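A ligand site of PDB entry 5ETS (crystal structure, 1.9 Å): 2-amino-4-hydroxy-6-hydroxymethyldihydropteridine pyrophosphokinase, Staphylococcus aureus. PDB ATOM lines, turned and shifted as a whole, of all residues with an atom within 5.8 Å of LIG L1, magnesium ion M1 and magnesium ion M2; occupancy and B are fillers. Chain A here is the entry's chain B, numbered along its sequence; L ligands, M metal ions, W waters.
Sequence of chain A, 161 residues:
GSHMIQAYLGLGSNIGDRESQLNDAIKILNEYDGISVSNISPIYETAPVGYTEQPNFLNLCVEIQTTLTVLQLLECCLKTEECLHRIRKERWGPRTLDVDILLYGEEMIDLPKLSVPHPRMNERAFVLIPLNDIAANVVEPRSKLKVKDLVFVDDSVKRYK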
ATOM      1  N   LEU A  74     -16.500  -9.305 -15.314  1.00  0.00           N
ATOM      2  CA  LEU A  74     -15.278  -9.965 -15.767  1.00  0.00           C
ATOM      3  C   LEU A  74     -15.460 -11.506 -15.711  1.00  0.00           C
ATOM      4  O   LEU A  74     -15.081 -12.196 -16.637  1.00  0.00           O
ATOM      5  CB  LEU A  74     -14.077  -9.547 -14.936  1.00  0.00           C
ATOM      6  CG  LEU A  74     -12.765 -10.272 -15.298  1.00  0.00           C
ATOM      7  CD1 LEU A  74     -12.304  -9.872 -16.719  1.00  0.00           C
ATOM      8  CD2 LEU A  74     -11.701 -10.001 -14.233  1.00  0.00           C
ATOM      9  N   LEU A  78     -14.923 -14.086 -18.966  1.00  0.00           N
ATOM     10  CA  LEU A  78     -13.968 -15.190 -18.953  1.00  0.00           C
ATOM     11  C   LEU A  78     -14.634 -16.554 -19.106  1.00  0.00           C
ATOM     12  O   LEU A  78     -14.096 -17.446 -19.770  1.00  0.00           O
ATOM     13  CB  LEU A  78     -13.123 -15.153 -17.675  1.00  0.00           C
ATOM     14  CG  LEU A  78     -12.286 -13.883 -17.504  1.00  0.00           C
ATOM     15  CD1 LEU A  78     -11.426 -13.964 -16.244  1.00  0.00           C
ATOM     16  CD2 LEU A  78     -11.386 -13.609 -18.693  1.00  0.00           C
ATOM     17  N   GLU A  81     -15.368 -17.112 -22.693  1.00  0.00           N
ATOM     18  CA  GLU A  81     -14.172 -17.593 -23.377  1.00  0.00           C
ATOM     19  C   GLU A  81     -13.961 -19.102 -23.197  1.00  0.00           C
ATOM     20  O   GLU A  81     -13.677 -19.828 -24.176  1.00  0.00           O
ATOM     21  CB  GLU A  81     -12.951 -16.836 -22.908  1.00  0.00           C
ATOM     22  CG  GLU A  81     -12.928 -15.381 -23.312  1.00  0.00           C
ATOM     23  CD  GLU A  81     -11.728 -14.659 -22.708  1.00  0.00           C
ATOM     24  OE1 GLU A  81     -11.081 -15.241 -21.800  1.00  0.00           O
ATOM     25  OE2 GLU A  81     -11.441 -13.522 -23.130  1.00  0.00           O
ATOM     26  N   ARG A  86     -11.300 -21.434 -25.522  1.00  0.00           N
ATOM     27  CA  ARG A  86     -10.053 -20.723 -25.640  1.00  0.00           C
ATOM     28  C   ARG A  86      -8.922 -21.480 -24.958  1.00  0.00           C
ATOM     29  O   ARG A  86      -9.048 -21.889 -23.820  1.00  0.00           O
ATOM     30  CB  ARG A  86     -10.161 -19.343 -25.055  1.00  0.00           C
ATOM     31  CG  ARG A  86      -8.792 -18.685 -25.027  1.00  0.00           C
ATOM     32  CD  ARG A  86      -8.959 -17.227 -25.066  1.00  0.00           C
ATOM     33  NE  ARG A  86      -7.716 -16.553 -24.827  1.00  0.00           N
ATOM     34  CZ  ARG A  86      -7.648 -15.257 -24.606  1.00  0.00           C
ATOM     35  NH1 ARG A  86      -8.763 -14.515 -24.580  1.00  0.00           N
ATOM     36  NH2 ARG A  86      -6.486 -14.685 -24.429  1.00  0.00           N
ATOM     37  N   ARG A  88      -5.036 -21.583 -23.538  1.00  0.00           N
ATOM     38  CA  ARG A  88      -4.077 -20.720 -22.871  1.00  0.00           C
ATOM     39  C   ARG A  88      -2.777 -21.503 -22.626  1.00  0.00           C
ATOM     40  O   ARG A  88      -2.675 -22.237 -21.698  1.00  0.00           O
ATOM     41  CB  ARG A  88      -4.626 -20.242 -21.582  1.00  0.00           C
ATOM     42  CG  ARG A  88      -6.092 -19.950 -21.613  1.00  0.00           C
ATOM     43  CD  ARG A  88      -6.453 -19.027 -20.475  1.00  0.00           C
ATOM     44  NE  ARG A  88      -5.586 -17.887 -20.513  1.00  0.00           N
ATOM     45  CZ  ARG A  88      -5.960 -16.711 -20.970  1.00  0.00           C
ATOM     46  NH1 ARG A  88      -7.199 -16.519 -21.362  1.00  0.00           N
ATOM     47  NH2 ARG A  88      -5.089 -15.758 -20.976  1.00  0.00           N
ATOM     48  N   ARG A  95      -6.563 -17.243 -30.764  1.00  0.00           N
ATOM     49  CA  ARG A  95      -7.607 -17.551 -29.795  1.00  0.00           C
ATOM     50  C   ARG A  95      -9.001 -17.621 -30.463  1.00  0.00           C
ATOM     51  O   ARG A  95      -9.344 -16.799 -31.340  1.00  0.00           O
ATOM     52  CB  ARG A  95      -7.611 -16.539 -28.642  1.00  0.00           C
ATOM     53  CG  ARG A  95      -7.895 -15.085 -29.024  1.00  0.00           C
ATOM     54  CD  ARG A  95      -6.685 -14.341 -29.589  1.00  0.00           C
ATOM     55  NE  ARG A  95      -5.500 -14.541 -28.782  1.00  0.00           N
ATOM     56  CZ  ARG A  95      -5.141 -13.785 -27.742  1.00  0.00           C
ATOM     57  NH1 ARG A  95      -5.839 -12.703 -27.369  1.00  0.00           N
ATOM     58  NH2 ARG A  95      -4.050 -14.141 -27.052  1.00  0.00           N
ATOM     59  N   ASP A  98     -11.756 -13.764 -27.429  1.00  0.00           N
ATOM     60  CA  ASP A  98     -11.268 -12.843 -26.473  1.00  0.00           C
ATOM     61  C   ASP A  98     -12.406 -11.872 -26.159  1.00  0.00           C
ATOM     62  O   ASP A  98     -12.961 -11.290 -27.059  1.00  0.00           O
ATOM     63  CB  ASP A  98     -10.055 -12.089 -27.019  1.00  0.00           C
ATOM     64  CG  ASP A  98      -9.422 -11.173 -25.982  1.00  0.00           C
ATOM     65  OD1 ASP A  98      -9.290 -11.566 -24.805  1.00  0.00           O
ATOM     66  OD2 ASP A  98      -9.057 -10.037 -26.357  1.00  0.00           O
ATOM     67  N   VAL A  99     -12.754 -11.749 -24.875  1.00  0.00           N
ATOM     68  CA  VAL A  99     -13.787 -10.816 -24.410  1.00  0.00           C
ATOM     69  C   VAL A  99     -13.150  -9.891 -23.404  1.00  0.00           C
ATOM     70  O   VAL A  99     -12.800 -10.299 -22.305  1.00  0.00           O
ATOM     71  CB  VAL A  99     -14.992 -11.512 -23.779  1.00  0.00           C
ATOM     72  CG1 VAL A  99     -16.091 -10.508 -23.463  1.00  0.00           C
ATOM     73  CG2 VAL A  99     -15.528 -12.603 -24.665  1.00  0.00           C
ATOM     74  N   ASP A 100     -13.018  -8.622 -23.796  1.00  0.00           N
ATOM     75  CA  ASP A 100     -12.343  -7.582 -23.009  1.00  0.00           C
ATOM     76  C   ASP A 100     -13.346  -6.517 -22.580  1.00  0.00           C
ATOM     77  O   ASP A 100     -14.105  -6.024 -23.382  1.00  0.00           O
ATOM     78  CB  ASP A 100     -11.242  -6.929 -23.839  1.00  0.00           C
ATOM     79  CG  ASP A 100     -10.068  -7.866 -24.130  1.00  0.00           C
ATOM     80  OD1 ASP A 100      -9.971  -8.950 -23.507  1.00  0.00           O
ATOM     81  OD2 ASP A 100      -9.185  -7.512 -24.954  1.00  0.00           O
ATOM     82  N   ILE A 101     -13.293  -6.119 -21.303  1.00  0.00           N
ATOM     83  CA  ILE A 101     -14.103  -5.008 -20.802  1.00  0.00           C
ATOM     84  C   ILE A 101     -13.388  -3.724 -21.194  1.00  0.00           C
ATOM     85  O   ILE A 101     -12.248  -3.462 -20.732  1.00  0.00           O
ATOM     86  CB  ILE A 101     -14.302  -5.054 -19.264  1.00  0.00           C
ATOM     87  CG1 ILE A 101     -15.006  -6.373 -18.833  1.00  0.00           C
ATOM     88  CG2 ILE A 101     -15.077  -3.801 -18.832  1.00  0.00           C
ATOM     89  CD1 ILE A 101     -14.953  -6.660 -17.359  1.00  0.00           C
ATOM     90  N   LEU A 102     -14.029  -2.937 -22.042  1.00  0.00           N
ATOM     91  CA  LEU A 102     -13.416  -1.684 -22.532  1.00  0.00           C
ATOM     92  C   LEU A 102     -13.756  -0.554 -21.611  1.00  0.00           C
ATOM     93  O   LEU A 102     -12.877   0.180 -21.196  1.00  0.00           O
ATOM     94  CB  LEU A 102     -13.893  -1.363 -23.952  1.00  0.00           C
ATOM     95  CG  LEU A 102     -13.568  -2.493 -24.948  1.00  0.00           C
ATOM     96  CD1 LEU A 102     -14.181  -2.162 -26.303  1.00  0.00           C
ATOM     97  CD2 LEU A 102     -12.066  -2.709 -25.109  1.00  0.00           C
ATOM     98  N   PRO A 112      -5.458  -5.853  -9.508  1.00  0.00           N
ATOM     99  CA  PRO A 112      -4.533  -6.825 -10.112  1.00  0.00           C
ATOM    100  C   PRO A 112      -5.149  -7.585 -11.286  1.00  0.00           C
ATOM    101  O   PRO A 112      -4.502  -7.713 -12.303  1.00  0.00           O
ATOM    102  CB  PRO A 112      -4.215  -7.759  -8.963  1.00  0.00           C
ATOM    103  CG  PRO A 112      -4.253  -6.849  -7.769  1.00  0.00           C
ATOM    104  CD  PRO A 112      -5.432  -5.933  -8.033  1.00  0.00           C
ATOM    105  N   LYS A 113      -6.356  -8.066 -11.146  1.00  0.00           N
ATOM    106  CA  LYS A 113      -6.958  -8.824 -12.235  1.00  0.00           C
ATOM    107  C   LYS A 113      -7.830  -8.050 -13.199  1.00  0.00           C
ATOM    108  O   LYS A 113      -8.431  -8.639 -14.026  1.00  0.00           O
ATOM    109  CB  LYS A 113      -7.713 -10.036 -11.666  1.00  0.00           C
ATOM    110  CG  LYS A 113      -9.052  -9.801 -10.980  1.00  0.00           C
ATOM    111  CD  LYS A 113      -9.638 -11.026 -10.221  1.00  0.00           C
ATOM    112  CE  LYS A 113     -10.182 -10.684  -8.847  1.00  0.00           C
ATOM    113  NZ  LYS A 113     -10.776 -11.758  -7.970  1.00  0.00           N
ATOM    114  N   LEU A 114      -7.866  -6.744 -13.083  1.00  0.00           N
ATOM    115  CA  LEU A 114      -8.813  -5.932 -13.851  1.00  0.00           C
ATOM    116  C   LEU A 114      -8.408  -4.463 -13.984  1.00  0.00           C
ATOM    117  O   LEU A 114      -8.288  -3.767 -12.992  1.00  0.00           O
ATOM    118  CB  LEU A 114     -10.198  -6.014 -13.224  1.00  0.00           C
ATOM    119  CG  LEU A 114     -11.313  -5.256 -13.955  1.00  0.00           C
ATOM    120  CD1 LEU A 114     -11.541  -5.767 -15.362  1.00  0.00           C
ATOM    121  CD2 LEU A 114     -12.569  -5.397 -13.138  1.00  0.00           C
ATOM    122  N   SER A 115      -8.290  -3.994 -15.227  1.00  0.00           N
ATOM    123  CA  SER A 115      -8.061  -2.584 -15.510  1.00  0.00           C
ATOM    124  C   SER A 115      -9.095  -2.132 -16.483  1.00  0.00           C
ATOM    125  O   SER A 115      -9.185  -2.656 -17.612  1.00  0.00           O
ATOM    126  CB  SER A 115      -6.679  -2.330 -16.093  1.00  0.00           C
ATOM    127  OG  SER A 115      -5.692  -2.873 -15.290  1.00  0.00           O
ATOM    128  N   VAL A 116      -9.853  -1.131 -16.057  1.00  0.00           N
ATOM    129  CA  VAL A 116     -10.905  -0.506 -16.867  1.00  0.00           C
ATOM    130  C   VAL A 116     -10.804   1.011 -16.666  1.00  0.00           C
ATOM    131  O   VAL A 116     -10.681   1.455 -15.517  1.00  0.00           O
ATOM    132  CB  VAL A 116     -12.278  -1.018 -16.435  1.00  0.00           C
ATOM    133  CG1 VAL A 116     -13.409  -0.313 -17.211  1.00  0.00           C
ATOM    134  CG2 VAL A 116     -12.358  -2.540 -16.589  1.00  0.00           C
ATOM    135  N   PRO A 117     -10.828   1.824 -17.705  1.00  0.00           N
ATOM    136  CA  PRO A 117     -10.870   1.418 -19.113  1.00  0.00           C
ATOM    137  C   PRO A 117      -9.683   0.536 -19.504  1.00  0.00           C
ATOM    138  O   PRO A 117      -8.616   0.636 -18.916  1.00  0.00           O
ATOM    139  CB  PRO A 117     -10.814   2.740 -19.870  1.00  0.00           C
ATOM    140  CG  PRO A 117     -11.434   3.701 -18.913  1.00  0.00           C
ATOM    141  CD  PRO A 117     -11.021   3.265 -17.550  1.00  0.00           C
ATOM    142  N   HIS A 118      -9.922  -0.347 -20.458  1.00  0.00           N
ATOM    143  CA  HIS A 118      -8.887  -1.244 -20.919  1.00  0.00           C
ATOM    144  C   HIS A 118      -7.632  -0.395 -21.193  1.00  0.00           C
ATOM    145  O   HIS A 118      -7.719   0.629 -21.836  1.00  0.00           O
ATOM    146  CB  HIS A 118      -9.339  -2.011 -22.152  1.00  0.00           C
ATOM    147  CG  HIS A 118      -8.380  -3.078 -22.537  1.00  0.00           C
ATOM    148  ND1 HIS A 118      -7.161  -2.802 -23.105  1.00  0.00           N
ATOM    149  CD2 HIS A 118      -8.408  -4.423 -22.318  1.00  0.00           C
ATOM    150  CE1 HIS A 118      -6.485  -3.932 -23.257  1.00  0.00           C
ATOM    151  NE2 HIS A 118      -7.232  -4.927 -22.806  1.00  0.00           N
ATOM    152  N   PRO A 119      -6.481  -0.788 -20.650  1.00  0.00           N
ATOM    153  CA  PRO A 119      -5.230  -0.001 -20.750  1.00  0.00           C
ATOM    154  C   PRO A 119      -4.660   0.319 -22.136  1.00  0.00           C
ATOM    155  O   PRO A 119      -3.879   1.243 -22.269  1.00  0.00           O
ATOM    156  CB  PRO A 119      -4.222  -0.799 -19.930  1.00  0.00           C
ATOM    157  CG  PRO A 119      -4.840  -2.113 -19.659  1.00  0.00           C
ATOM    158  CD  PRO A 119      -6.328  -1.960 -19.774  1.00  0.00           C
ATOM    159  N   ARG A 120      -5.048  -0.452 -23.128  1.00  0.00           N
ATOM    160  CA  ARG A 120      -4.573  -0.248 -24.524  1.00  0.00           C
ATOM    161  C   ARG A 120      -5.586   0.305 -25.510  1.00  0.00           C
ATOM    162  O   ARG A 120      -5.228   0.542 -26.677  1.00  0.00           O
ATOM    163  CB  ARG A 120      -3.936  -1.566 -25.035  1.00  0.00           C
ATOM    164  CG  ARG A 120      -2.599  -1.882 -24.365  1.00  0.00           C
ATOM    165  CD  ARG A 120      -2.119  -3.331 -24.544  1.00  0.00           C
ATOM    166  NE  ARG A 120      -2.831  -4.264 -23.683  1.00  0.00           N
ATOM    167  CZ  ARG A 120      -2.634  -4.397 -22.362  1.00  0.00           C
ATOM    168  NH1 ARG A 120      -1.743  -3.647 -21.700  1.00  0.00           N
ATOM    169  NH2 ARG A 120      -3.370  -5.256 -21.683  1.00  0.00           N
ATOM    170  N   ARG A 124      -5.762   1.601 -30.184  1.00  0.00           N
ATOM    171  CA  ARG A 124      -6.111   0.416 -30.975  1.00  0.00           C
ATOM    172  C   ARG A 124      -7.249   0.721 -31.934  1.00  0.00           C
ATOM    173  O   ARG A 124      -8.409   0.855 -31.506  1.00  0.00           O
ATOM    174  CB  ARG A 124      -6.512  -0.731 -30.047  1.00  0.00           C
ATOM    175  CG  ARG A 124      -5.312  -1.416 -29.425  1.00  0.00           C
ATOM    176  CD  ARG A 124      -5.706  -2.385 -28.309  1.00  0.00           C
ATOM    177  NE  ARG A 124      -4.635  -3.327 -28.032  1.00  0.00           N
ATOM    178  CZ  ARG A 124      -4.769  -4.438 -27.315  1.00  0.00           C
ATOM    179  NH1 ARG A 124      -5.901  -4.723 -26.708  1.00  0.00           N
ATOM    180  NH2 ARG A 124      -3.726  -5.264 -27.187  1.00  0.00           N
ATOM    181  N   PHE A 126      -8.581  -1.437 -33.875  1.00  0.00           N
ATOM    182  CA  PHE A 126      -9.477  -2.579 -33.873  1.00  0.00           C
ATOM    183  C   PHE A 126     -10.538  -2.491 -32.776  1.00  0.00           C
ATOM    184  O   PHE A 126     -11.549  -3.205 -32.838  1.00  0.00           O
ATOM    185  CB  PHE A 126      -8.723  -3.933 -33.859  1.00  0.00           C
ATOM    186  CG  PHE A 126      -8.154  -4.331 -32.542  1.00  0.00           C
ATOM    187  CD1 PHE A 126      -8.962  -4.893 -31.545  1.00  0.00           C
ATOM    188  CD2 PHE A 126      -6.799  -4.187 -32.286  1.00  0.00           C
ATOM    189  CE1 PHE A 126      -8.434  -5.282 -30.322  1.00  0.00           C
ATOM    190  CE2 PHE A 126      -6.265  -4.568 -31.063  1.00  0.00           C
ATOM    191  CZ  PHE A 126      -7.079  -5.126 -30.078  1.00  0.00           C
HETATM  192  P1  LIG L   1      -5.133  -7.359 -24.255  1.00  0.00           P
HETATM  193  O1  LIG L   1      -6.324  -7.246 -25.183  1.00  0.00           O
HETATM  194  O2  LIG L   1      -3.876  -6.656 -24.701  1.00  0.00           O
HETATM  195  O3  LIG L   1      -5.496  -7.040 -22.831  1.00  0.00           O
HETATM  196  P2  LIG L   1      -5.681 -10.219 -24.001  1.00  0.00           P
HETATM  197  O4  LIG L   1      -5.226 -11.342 -24.881  1.00  0.00           O
HETATM  198  O5  LIG L   1      -7.098  -9.706 -24.059  1.00  0.00           O
HETATM  199  O6  LIG L   1      -4.698  -8.941 -24.194  1.00  0.00           O
HETATM  200  P3  LIG L   1      -6.222 -12.184 -21.766  1.00  0.00           P
HETATM  201  O7  LIG L   1      -7.524 -12.161 -22.515  1.00  0.00           O
HETATM  202  O8  LIG L   1      -5.304 -13.363 -21.873  1.00  0.00           O
HETATM  203  C1  LIG L   1      -5.375 -10.670 -22.284  1.00  0.00           C
HETATM  204  O9  LIG L   1      -6.637 -11.887 -20.204  1.00  0.00           O
HETATM  205  C2  LIG L   1      -5.713 -12.049 -19.136  1.00  0.00           C
HETATM  206  C3  LIG L   1      -6.267 -11.435 -17.850  1.00  0.00           C
HETATM  207  O10 LIG L   1      -6.411 -10.035 -18.061  1.00  0.00           O
HETATM  208  C4  LIG L   1      -7.676 -11.851 -17.473  1.00  0.00           C
HETATM  209  O11 LIG L   1      -7.651 -13.070 -16.737  1.00  0.00           O
HETATM  210  C5  LIG L   1      -8.193 -10.675 -16.676  1.00  0.00           C
HETATM  211  O12 LIG L   1      -8.146 -10.929 -15.261  1.00  0.00           O
HETATM  212  C6  LIG L   1      -7.229  -9.551 -17.003  1.00  0.00           C
HETATM  213  N1  LIG L   1      -7.858  -8.288 -17.411  1.00  0.00           N
HETATM  214  C7  LIG L   1      -7.408  -7.057 -17.000  1.00  0.00           C
HETATM  215  N2  LIG L   1      -8.150  -6.080 -17.476  1.00  0.00           N
HETATM  216  C8  LIG L   1      -9.111  -6.716 -18.243  1.00  0.00           C
HETATM  217  C9  LIG L   1     -10.169  -6.217 -18.991  1.00  0.00           C
HETATM  218  N3  LIG L   1     -10.399  -4.837 -19.081  1.00  0.00           N
HETATM  219  N4  LIG L   1     -10.958  -7.093 -19.632  1.00  0.00           N
HETATM  220  C10 LIG L   1     -10.701  -8.405 -19.528  1.00  0.00           C
HETATM  221  N5  LIG L   1      -9.717  -8.998 -18.840  1.00  0.00           N
HETATM  222  C11 LIG L   1      -8.958  -8.083 -18.212  1.00  0.00           C
HETATM  223  C1  LG2 L   2      -1.750 -10.595 -30.956  1.00  0.00           C
HETATM  224  C2  LG2 L   2      -1.895 -11.885 -28.983  1.00  0.00           C
HETATM  225  C3  LG2 L   2      -1.942 -11.731 -31.725  1.00  0.00           C
HETATM  226  C4  LG2 L   2      -2.080 -13.026 -29.749  1.00  0.00           C
HETATM  227  C5  LG2 L   2      -1.732 -10.641 -29.571  1.00  0.00           C
HETATM  228  C6  LG2 L   2      -5.853  -8.183 -30.615  1.00  0.00           C
HETATM  229  C7  LG2 L   2      -2.108 -12.959 -31.129  1.00  0.00           C
HETATM  230  C8  LG2 L   2      -4.785  -7.765 -31.341  1.00  0.00           C
HETATM  231  C9  LG2 L   2      -7.154  -8.188 -31.235  1.00  0.00           C
HETATM  232  C10 LG2 L   2      -5.896  -7.336 -33.183  1.00  0.00           C
HETATM  233  C11 LG2 L   2      -4.179  -8.341 -29.305  1.00  0.00           C
HETATM  234  C12 LG2 L   2      -1.560  -9.397 -28.711  1.00  0.00           C
HETATM  235  N1  LG2 L   2      -4.729  -7.336 -32.620  1.00  0.00           N
HETATM  236  N2  LG2 L   2      -3.723  -7.873 -30.502  1.00  0.00           N
HETATM  237  N3  LG2 L   2      -7.072  -7.740 -32.544  1.00  0.00           N
HETATM  238  N4  LG2 L   2      -5.489  -8.538 -29.347  1.00  0.00           N
HETATM  239  N5  LG2 L   2      -6.085  -6.933 -34.486  1.00  0.00           N
HETATM  240  O1  LG2 L   2      -8.196  -8.522 -30.695  1.00  0.00           O
HETATM  241  S1  LG2 L   2      -3.086  -8.622 -27.956  1.00  0.00           S
HETATM  242 CL1  LG2 L   2      -2.360 -14.410 -32.074  1.00  0.00          CL
HETATM  243 MG    MG M   1      -7.672  -8.591 -25.837  1.00  0.00          MG
HETATM  244 MG    MG M   2      -8.662 -10.503 -23.070  1.00  0.00          MG
HETATM  245  O   HOH W   1      -4.006  -8.996 -19.316  1.00  0.00           O
HETATM  246  O   HOH W   2     -10.286 -11.329 -21.974  1.00  0.00           O
HETATM  247  O   HOH W   3      -8.242  -9.553 -21.285  1.00  0.00           O
HETATM  248  O   HOH W   4      -6.430  -7.618 -20.390  1.00  0.00           O
HETATM  249  O   HOH W   5      -8.830 -14.181 -20.961  1.00  0.00           O
HETATM  250  O   HOH W   6      -6.225  -5.257 -19.616  1.00  0.00           O
HETATM  251  O   HOH W   7      -7.771 -15.066 -18.557  1.00  0.00           O
HETATM  252  O   HOH W   8      -8.036  -7.538 -27.665  1.00  0.00           O
HETATM  253  O   HOH W   9      -6.247  -9.647 -26.958  1.00  0.00           O
HETATM  254  O   HOH W  10      -1.524  -7.866 -23.752  1.00  0.00           O
HETATM  255  O   HOH W  11      -8.675 -13.297 -13.990  1.00  0.00           O
HETATM  256  O   HOH W  12      -2.688 -12.311 -25.185  1.00  0.00           O
HETATM  257  O   HOH W  13      -3.032 -13.826 -22.996  1.00  0.00           O
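Magnesium ion M1 is bound by O1 of LIG L1, OD2 of Asp 100, OD2 of Asp 98, water W9, water W8 and O5 of LIG L1.
O5 of LIG L1 binds magnesium ion M2, 2.0 Å away.
Water W3 is bound to magnesium ion M2 (2.1 Å).
Magnesium ion M2 is bound by OD1 of Asp 100, 2.1 Å away.
O7 of LIG L1 binds magnesium ion M2, at 2.1 Å.
Magnesium ion M2 is bound by water W2 (2.1 Å).
OD1 of Asp 98 is bound to magnesium ion M2 (2.1 Å).
Magnesium ion M2 has six donor atoms within binding distance.
The guanidinium group (NH1) of Arg 86 lies within salt-bridge range of the side-chain carboxylate (OE2) of Glu 81 (3.2 Å).
NH1 of Arg 86 lies close to OD1 of Asp 98, 3.0 Å away.
N of His 118 lies within hydrogen-bond range of O of Leu 102 (3.1 Å).
The backbone NH of Arg 120 lies within hydrogen-bond range of a ring nitrogen (ND1) of His 118 (3.2 Å).
The side-chain carboxylate of Glu 81 sits at hydrogen-bond distance from the backbone NH of Val 99, at 2.8 Å.
Water W9 lies within hydrogen-bond range of N4 of LG2 L2, O4 of LIG L1 and NH1 of Arg 95.
Water W2 lies within hydrogen-bond range of the side-chain carboxylate (OE2) of Glu 81 and the backbone carbonyl oxygen (O) of Val 99.
Water W13 bridges O8 of LIG L1 (2.6 Å) and NH2 of Arg 88 (3.5 Å).
Water W7 bridges an oxygen (O11) of LIG L1 (2.7 Å) and the guanidinium group of Arg 88 (3.2 Å).
Water W12 bridges O4 of LIG L1 (2.7 Å) and NH2 of Arg 95 (2.9 Å).
Water W5 lies within hydrogen-bond range of the side-chain carboxylate of Glu 81, the guanidinium group of Arg 88 and an oxygen (O9) of LIG L1.
The nearest printed residue that does not touch magnesium ion M1 is Arg 124 (4.3 Å).
Of the 22 residues printed, 2 come within 4 Å of magnesium ion M2.
Merely in contact with LIG L1: Leu 74, Leu 78, Val 99, Leu 114 and Val 116.
Of the 22 residues printed, 16 come within 4 Å of LIG L1.
The nearest printed residue that does not touch LIG L1 is Glu 81 (4.2 Å).
The backbone carbonyl oxygen (O) of Ser 115 sits at hydrogen-bond distance from a nitrogen (N3) of LIG L1, at 2.9 Å.
O8 of LIG L1 is in salt-bridge range of NH2 of Arg 86, 3.1 Å away.
O3 of LIG L1 lies within hydrogen-bond range of NE2 of His 118 (2.7 Å).
The guanidinium group (NH1) of Arg 95 is in salt-bridge range of an oxygen (O4) of LIG L1 (2.9 Å).
An oxygen (O2) of LIG L1 lies within salt-bridge range of the guanidinium group of Arg 120 (2.8 Å).
NH2 of Arg 124 lies within salt-bridge range of O2 of LIG L1, at 2.9 Å.
An oxygen (O12) of LIG L1 is in hydrogen-bond range of the backbone carbonyl oxygen of Lys 113.
The backbone NH of Ile 101 lies within hydrogen-bond range of a nitrogen (N4) of LIG L1.
O of Ile 101 sits at hydrogen-bond distance from N3 of LIG L1 (2.8 Å).
N of Ser 115 is in hydrogen-bond range of N2 of LIG L1 (3.1 Å).
The guanidinium group (NH2) of Arg 88 is in salt-bridge range of an oxygen (O8) of LIG L1, at 2.6 Å.
The guanidinium group (NH2) of Arg 124 sits close to a sulfur (S1) of LG2 L2 (3.5 Å).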
